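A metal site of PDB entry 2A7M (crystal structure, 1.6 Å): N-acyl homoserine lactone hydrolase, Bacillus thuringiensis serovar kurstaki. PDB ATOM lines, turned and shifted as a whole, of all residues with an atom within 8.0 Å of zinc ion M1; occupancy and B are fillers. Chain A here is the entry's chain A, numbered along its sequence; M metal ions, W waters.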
ATOM      1  N   LEU A  16     -32.103 -21.072  16.560  1.00  0.00           N
ATOM      2  CA  LEU A  16     -32.882 -20.310  17.532  1.00  0.00           C
ATOM      3  C   LEU A  16     -34.085 -19.773  16.793  1.00  0.00           C
ATOM      4  O   LEU A  16     -34.030 -19.601  15.579  1.00  0.00           O
ATOM      5  CB  LEU A  16     -32.071 -19.148  18.113  1.00  0.00           C
ATOM      6  CG  LEU A  16     -31.039 -19.461  19.200  1.00  0.00           C
ATOM      7  CD1 LEU A  16     -29.718 -19.886  18.596  1.00  0.00           C
ATOM      8  CD2 LEU A  16     -30.830 -18.243  20.073  1.00  0.00           C
ATOM      9  N   ASP A  50     -13.732 -18.310  23.455  1.00  0.00           N
ATOM     10  CA  ASP A  50     -14.869 -19.234  23.465  1.00  0.00           C
ATOM     11  C   ASP A  50     -14.522 -20.635  22.971  1.00  0.00           C
ATOM     12  O   ASP A  50     -13.492 -20.839  22.318  1.00  0.00           O
ATOM     13  CB  ASP A  50     -16.122 -18.610  22.800  1.00  0.00           C
ATOM     14  CG  ASP A  50     -16.695 -17.441  23.608  1.00  0.00           C
ATOM     15  OD1 ASP A  50     -16.341 -17.299  24.800  1.00  0.00           O
ATOM     16  OD2 ASP A  50     -17.483 -16.657  23.034  1.00  0.00           O
ATOM     17  N   SER A 103     -16.308 -15.221  26.709  1.00  0.00           N
ATOM     18  CA  SER A 103     -17.157 -14.026  26.592  1.00  0.00           C
ATOM     19  C   SER A 103     -18.310 -14.091  27.600  1.00  0.00           C
ATOM     20  O   SER A 103     -18.656 -13.095  28.229  1.00  0.00           O
ATOM     21  CB  SER A 103     -17.722 -13.894  25.197  1.00  0.00           C
ATOM     22  OG  SER A 103     -18.495 -15.026  24.881  1.00  0.00           O
ATOM     23  N   HIS A 104     -18.895 -15.282  27.713  1.00  0.00           N
ATOM     24  CA  HIS A 104     -19.903 -15.584  28.704  1.00  0.00           C
ATOM     25  C   HIS A 104     -20.056 -17.101  28.782  1.00  0.00           C
ATOM     26  O   HIS A 104     -19.346 -17.828  28.048  1.00  0.00           O
ATOM     27  CB  HIS A 104     -21.224 -14.824  28.432  1.00  0.00           C
ATOM     28  CG  HIS A 104     -21.898 -15.130  27.131  1.00  0.00           C
ATOM     29  ND1 HIS A 104     -21.284 -15.067  25.898  1.00  0.00           N
ATOM     30  CD2 HIS A 104     -23.201 -15.401  26.879  1.00  0.00           C
ATOM     31  CE1 HIS A 104     -22.171 -15.307  24.949  1.00  0.00           C
ATOM     32  NE2 HIS A 104     -23.346 -15.532  25.517  1.00  0.00           N
ATOM     33  N   LEU A 105     -20.920 -17.586  29.661  1.00  0.00           N
ATOM     34  CA  LEU A 105     -20.983 -19.024  29.904  1.00  0.00           C
ATOM     35  C   LEU A 105     -22.233 -19.703  29.336  1.00  0.00           C
ATOM     36  O   LEU A 105     -22.594 -20.817  29.747  1.00  0.00           O
ATOM     37  CB  LEU A 105     -20.767 -19.314  31.400  1.00  0.00           C
ATOM     38  CG  LEU A 105     -19.392 -18.923  31.973  1.00  0.00           C
ATOM     39  CD1 LEU A 105     -19.309 -19.211  33.478  1.00  0.00           C
ATOM     40  CD2 LEU A 105     -18.202 -19.559  31.231  1.00  0.00           C
ATOM     41  N   HIS A 106     -22.894 -19.052  28.377  1.00  0.00           N
ATOM     42  CA  HIS A 106     -23.934 -19.719  27.628  1.00  0.00           C
ATOM     43  C   HIS A 106     -23.349 -20.932  26.907  1.00  0.00           C
ATOM     44  O   HIS A 106     -22.155 -20.980  26.615  1.00  0.00           O
ATOM     45  CB  HIS A 106     -24.570 -18.778  26.606  1.00  0.00           C
ATOM     46  CG  HIS A 106     -25.481 -17.760  27.223  1.00  0.00           C
ATOM     47  ND1 HIS A 106     -26.008 -16.697  26.487  1.00  0.00           N
ATOM     48  CD2 HIS A 106     -25.971 -17.626  28.479  1.00  0.00           C
ATOM     49  CE1 HIS A 106     -26.756 -15.955  27.289  1.00  0.00           C
ATOM     50  NE2 HIS A 106     -26.756 -16.498  28.496  1.00  0.00           N
ATOM     51  N   PHE A 107     -24.208 -21.898  26.639  1.00  0.00           N
ATOM     52  CA  PHE A 107     -23.772 -23.219  26.157  1.00  0.00           C
ATOM     53  C   PHE A 107     -23.045 -23.203  24.803  1.00  0.00           C
ATOM     54  O   PHE A 107     -22.233 -24.093  24.513  1.00  0.00           O
ATOM     55  CB  PHE A 107     -24.959 -24.193  26.123  1.00  0.00           C
ATOM     56  CG  PHE A 107     -25.625 -24.320  24.773  1.00  0.00           C
ATOM     57  CD1 PHE A 107     -25.479 -25.492  24.031  1.00  0.00           C
ATOM     58  CD2 PHE A 107     -26.353 -23.272  24.229  1.00  0.00           C
ATOM     59  CE1 PHE A 107     -26.076 -25.619  22.774  1.00  0.00           C
ATOM     60  CE2 PHE A 107     -26.947 -23.388  22.963  1.00  0.00           C
ATOM     61  CZ  PHE A 107     -26.793 -24.555  22.244  1.00  0.00           C
ATOM     62  N   ASP A 108     -23.353 -22.193  23.982  1.00  0.00           N
ATOM     63  CA  ASP A 108     -22.698 -22.052  22.673  1.00  0.00           C
ATOM     64  C   ASP A 108     -21.355 -21.326  22.752  1.00  0.00           C
ATOM     65  O   ASP A 108     -20.705 -21.154  21.731  1.00  0.00           O
ATOM     66  CB  ASP A 108     -23.644 -21.401  21.640  1.00  0.00           C
ATOM     67  CG  ASP A 108     -24.239 -20.070  22.098  1.00  0.00           C
ATOM     68  OD1 ASP A 108     -24.241 -19.125  21.286  1.00  0.00           O
ATOM     69  OD2 ASP A 108     -24.719 -19.955  23.262  1.00  0.00           O
ATOM     70  N   HIS A 109     -20.925 -20.952  23.973  1.00  0.00           N
ATOM     71  CA  HIS A 109     -19.672 -20.225  24.192  1.00  0.00           C
ATOM     72  C   HIS A 109     -18.721 -20.898  25.162  1.00  0.00           C
ATOM     73  O   HIS A 109     -17.511 -20.664  25.089  1.00  0.00           O
ATOM     74  CB  HIS A 109     -20.010 -18.816  24.699  1.00  0.00           C
ATOM     75  CG  HIS A 109     -20.813 -18.043  23.702  1.00  0.00           C
ATOM     76  ND1 HIS A 109     -20.224 -17.199  22.784  1.00  0.00           N
ATOM     77  CD2 HIS A 109     -22.129 -18.073  23.406  1.00  0.00           C
ATOM     78  CE1 HIS A 109     -21.160 -16.703  21.989  1.00  0.00           C
ATOM     79  NE2 HIS A 109     -22.334 -17.216  22.359  1.00  0.00           N
ATOM     80  N   GLU A 127     -20.464 -13.153  35.659  1.00  0.00           N
ATOM     81  CA  GLU A 127     -20.925 -14.246  34.814  1.00  0.00           C
ATOM     82  C   GLU A 127     -20.747 -15.565  35.557  1.00  0.00           C
ATOM     83  O   GLU A 127     -21.650 -16.404  35.572  1.00  0.00           O
ATOM     84  CB  GLU A 127     -20.113 -14.288  33.527  1.00  0.00           C
ATOM     85  CG  GLU A 127     -20.607 -15.334  32.519  1.00  0.00           C
ATOM     86  CD  GLU A 127     -21.966 -15.019  31.892  1.00  0.00           C
ATOM     87  OE1 GLU A 127     -22.442 -13.862  31.981  1.00  0.00           O
ATOM     88  OE2 GLU A 127     -22.554 -15.941  31.313  1.00  0.00           O
ATOM     89  N   TYR A 137     -28.058 -21.936  32.578  1.00  0.00           N
ATOM     90  CA  TYR A 137     -26.688 -22.458  32.489  1.00  0.00           C
ATOM     91  C   TYR A 137     -26.592 -23.968  32.615  1.00  0.00           C
ATOM     92  O   TYR A 137     -27.182 -24.587  33.520  1.00  0.00           O
ATOM     93  CB  TYR A 137     -25.781 -21.761  33.496  1.00  0.00           C
ATOM     94  CG  TYR A 137     -25.581 -20.305  33.164  1.00  0.00           C
ATOM     95  CD1 TYR A 137     -26.430 -19.319  33.674  1.00  0.00           C
ATOM     96  CD2 TYR A 137     -24.577 -19.917  32.284  1.00  0.00           C
ATOM     97  CE1 TYR A 137     -26.246 -17.975  33.356  1.00  0.00           C
ATOM     98  CE2 TYR A 137     -24.384 -18.584  31.966  1.00  0.00           C
ATOM     99  CZ  TYR A 137     -25.230 -17.631  32.493  1.00  0.00           C
ATOM    100  OH  TYR A 137     -25.047 -16.316  32.161  1.00  0.00           O
ATOM    101  N   HIS A 169     -26.872  -9.085  27.841  1.00  0.00           N
ATOM    102  CA  HIS A 169     -27.227 -10.336  27.187  1.00  0.00           C
ATOM    103  C   HIS A 169     -27.114 -11.492  28.184  1.00  0.00           C
ATOM    104  O   HIS A 169     -27.921 -12.408  28.174  1.00  0.00           O
ATOM    105  CB  HIS A 169     -26.314 -10.596  26.000  1.00  0.00           C
ATOM    106  CG  HIS A 169     -26.466 -11.977  25.453  1.00  0.00           C
ATOM    107  ND1 HIS A 169     -27.598 -12.401  24.781  1.00  0.00           N
ATOM    108  CD2 HIS A 169     -25.614 -13.034  25.454  1.00  0.00           C
ATOM    109  CE1 HIS A 169     -27.443 -13.657  24.417  1.00  0.00           C
ATOM    110  NE2 HIS A 169     -26.235 -14.063  24.796  1.00  0.00           N
ATOM    111  N   SER A 170     -26.060 -11.445  29.003  1.00  0.00           N
ATOM    112  CA  SER A 170     -25.912 -12.311  30.163  1.00  0.00           C
ATOM    113  C   SER A 170     -25.317 -11.411  31.260  1.00  0.00           C
ATOM    114  O   SER A 170     -24.783 -10.331  30.963  1.00  0.00           O
ATOM    115  CB  SER A 170     -24.997 -13.507  29.872  1.00  0.00           C
ATOM    116  OG  SER A 170     -23.639 -13.084  29.712  1.00  0.00           O
ATOM    117  N   HIS A 173     -21.494 -10.680  30.617  1.00  0.00           N
ATOM    118  CA  HIS A 173     -21.012 -10.766  29.243  1.00  0.00           C
ATOM    119  C   HIS A 173     -19.856  -9.773  29.010  1.00  0.00           C
ATOM    120  O   HIS A 173     -19.884  -8.642  29.521  1.00  0.00           O
ATOM    121  CB  HIS A 173     -22.145 -10.516  28.245  1.00  0.00           C
ATOM    122  CG  HIS A 173     -21.676 -10.513  26.830  1.00  0.00           C
ATOM    123  ND1 HIS A 173     -21.737 -11.632  26.012  1.00  0.00           N
ATOM    124  CD2 HIS A 173     -21.058  -9.556  26.103  1.00  0.00           C
ATOM    125  CE1 HIS A 173     -21.203 -11.335  24.835  1.00  0.00           C
ATOM    126  NE2 HIS A 173     -20.793 -10.084  24.867  1.00  0.00           N
ATOM    127  N   ILE A 190     -19.200  -9.992  20.301  1.00  0.00           N
ATOM    128  CA  ILE A 190     -19.784 -11.264  20.710  1.00  0.00           C
ATOM    129  C   ILE A 190     -21.265 -11.046  20.878  1.00  0.00           C
ATOM    130  O   ILE A 190     -21.883 -10.451  20.000  1.00  0.00           O
ATOM    131  CB  ILE A 190     -19.108 -11.867  21.972  1.00  0.00           C
ATOM    132  CG1 ILE A 190     -17.578 -11.614  21.951  1.00  0.00           C
ATOM    133  CG2 ILE A 190     -19.456 -13.358  22.085  1.00  0.00           C
ATOM    134  CD1 ILE A 190     -16.791 -12.406  20.895  1.00  0.00           C
ATOM    135  N   ASP A 191     -21.867 -11.477  21.976  1.00  0.00           N
ATOM    136  CA  ASP A 191     -23.327 -11.423  22.066  1.00  0.00           C
ATOM    137  C   ASP A 191     -23.893 -10.113  22.659  1.00  0.00           C
ATOM    138  O   ASP A 191     -25.066 -10.049  23.038  1.00  0.00           O
ATOM    139  CB  ASP A 191     -23.888 -12.668  22.777  1.00  0.00           C
ATOM    140  CG  ASP A 191     -23.753 -13.957  21.927  1.00  0.00           C
ATOM    141  OD1 ASP A 191     -23.123 -13.918  20.856  1.00  0.00           O
ATOM    142  OD2 ASP A 191     -24.272 -15.025  22.350  1.00  0.00           O
ATOM    143  N   ALA A 192     -23.072  -9.060  22.698  1.00  0.00           N
ATOM    144  CA  ALA A 192     -23.562  -7.727  23.060  1.00  0.00           C
ATOM    145  C   ALA A 192     -24.415  -7.182  21.917  1.00  0.00           C
ATOM    146  O   ALA A 192     -25.135  -6.201  22.069  1.00  0.00           O
ATOM    147  CB  ALA A 192     -22.390  -6.793  23.393  1.00  0.00           C
ATOM    148  N   TYR A 194     -26.270  -9.661  18.602  1.00  0.00           N
ATOM    149  CA  TYR A 194     -26.289 -10.800  17.676  1.00  0.00           C
ATOM    150  C   TYR A 194     -26.043 -10.334  16.242  1.00  0.00           C
ATOM    151  O   TYR A 194     -25.257 -10.938  15.514  1.00  0.00           O
ATOM    152  CB  TYR A 194     -27.638 -11.523  17.719  1.00  0.00           C
ATOM    153  CG  TYR A 194     -27.838 -12.493  18.874  1.00  0.00           C
ATOM    154  CD1 TYR A 194     -27.005 -12.504  19.988  1.00  0.00           C
ATOM    155  CD2 TYR A 194     -28.902 -13.378  18.839  1.00  0.00           C
ATOM    156  CE1 TYR A 194     -27.221 -13.396  21.029  1.00  0.00           C
ATOM    157  CE2 TYR A 194     -29.135 -14.256  19.868  1.00  0.00           C
ATOM    158  CZ  TYR A 194     -28.298 -14.255  20.964  1.00  0.00           C
ATOM    159  OH  TYR A 194     -28.559 -15.147  21.967  1.00  0.00           O
ATOM    160  N   PHE A 205     -33.024  -7.969  21.354  1.00  0.00           N
ATOM    161  CA  PHE A 205     -32.695  -9.366  21.072  1.00  0.00           C
ATOM    162  C   PHE A 205     -32.587 -10.147  22.379  1.00  0.00           C
ATOM    163  O   PHE A 205     -32.691  -9.564  23.453  1.00  0.00           O
ATOM    164  CB  PHE A 205     -31.403  -9.462  20.238  1.00  0.00           C
ATOM    165  CG  PHE A 205     -30.154  -9.009  20.973  1.00  0.00           C
ATOM    166  CD1 PHE A 205     -29.254  -9.939  21.486  1.00  0.00           C
ATOM    167  CD2 PHE A 205     -29.870  -7.650  21.130  1.00  0.00           C
ATOM    168  CE1 PHE A 205     -28.093  -9.518  22.162  1.00  0.00           C
ATOM    169  CE2 PHE A 205     -28.715  -7.216  21.787  1.00  0.00           C
ATOM    170  CZ  PHE A 205     -27.827  -8.156  22.307  1.00  0.00           C
ATOM    171  N   ALA A 206     -32.415 -11.470  22.265  1.00  0.00           N
ATOM    172  CA  ALA A 206     -32.341 -12.369  23.420  1.00  0.00           C
ATOM    173  C   ALA A 206     -31.333 -11.880  24.458  1.00  0.00           C
ATOM    174  O   ALA A 206     -30.194 -11.540  24.113  1.00  0.00           O
ATOM    175  CB  ALA A 206     -31.947 -13.768  22.953  1.00  0.00           C
ATOM    176  N   GLY A 207     -31.770 -11.803  25.715  1.00  0.00           N
ATOM    177  CA  GLY A 207     -30.859 -11.411  26.788  1.00  0.00           C
ATOM    178  C   GLY A 207     -31.485 -11.410  28.160  1.00  0.00           C
ATOM    179  O   GLY A 207     -32.707 -11.268  28.307  1.00  0.00           O
ATOM    180  N   HIS A 235     -23.918 -13.422  16.129  1.00  0.00           N
ATOM    181  CA  HIS A 235     -24.713 -14.481  15.523  1.00  0.00           C
ATOM    182  C   HIS A 235     -25.427 -13.890  14.304  1.00  0.00           C
ATOM    183  O   HIS A 235     -26.674 -13.820  14.265  1.00  0.00           O
ATOM    184  CB  HIS A 235     -25.735 -15.046  16.521  1.00  0.00           C
ATOM    185  CG  HIS A 235     -25.148 -15.836  17.666  1.00  0.00           C
ATOM    186  ND1 HIS A 235     -24.517 -17.050  17.502  1.00  0.00           N
ATOM    187  CD2 HIS A 235     -25.146 -15.584  19.001  1.00  0.00           C
ATOM    188  CE1 HIS A 235     -24.125 -17.498  18.679  1.00  0.00           C
ATOM    189  NE2 HIS A 235     -24.497 -16.631  19.604  1.00  0.00           N
HETATM  190 ZN    ZN M   1     -25.217 -15.872  24.671  1.00  0.00          ZN
HETATM  191 ZN    ZN M   2     -24.206 -16.908  21.673  1.00  0.00          ZN
HETATM  192  O   HOH W   1     -25.494 -17.225  23.139  1.00  0.00           O
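Merely in contact with zinc ion M1: His 109 (3.9 Å).
Of the 22 residues printed, 5 come within 4 Å of zinc ion M1.
Water W1 binds zinc ion M1 (2.1 Å).
Zinc ion M1 is bound by a ring nitrogen (NE2) of His 169.
NE2 of His 104 is bound to zinc ion M1 (2.1 Å).
ND1 of His 106 binds zinc ion M1.
Slightly farther from zinc ion M1 lies OD2 of Asp 191 (2.6 Å).
A ring nitrogen (ND1) of His 104 is in hydrogen-bond range of a ring nitrogen (ND1) of His 173 (3.5 Å).
The side-chain carboxylate (OD2) of Asp 50 lies within hydrogen-bond range of a ring nitrogen (ND1) of His 109 (2.8 Å).
ND1 of His 109 lies within hydrogen-bond range of OG of Ser 103, at 3.5 Å.
The backbone carbonyl oxygen (O) of Ala 206 lies within hydrogen-bond range of a ring nitrogen (ND1) of His 169 (2.8 Å).
A ring nitrogen (ND1) of His 104 lies within hydrogen-bond range of the side-chain hydroxyl (OG) of Ser 103, 3.0 Å away.
N of Asp 191 lies close to NE2 of His 173 (3.4 Å).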
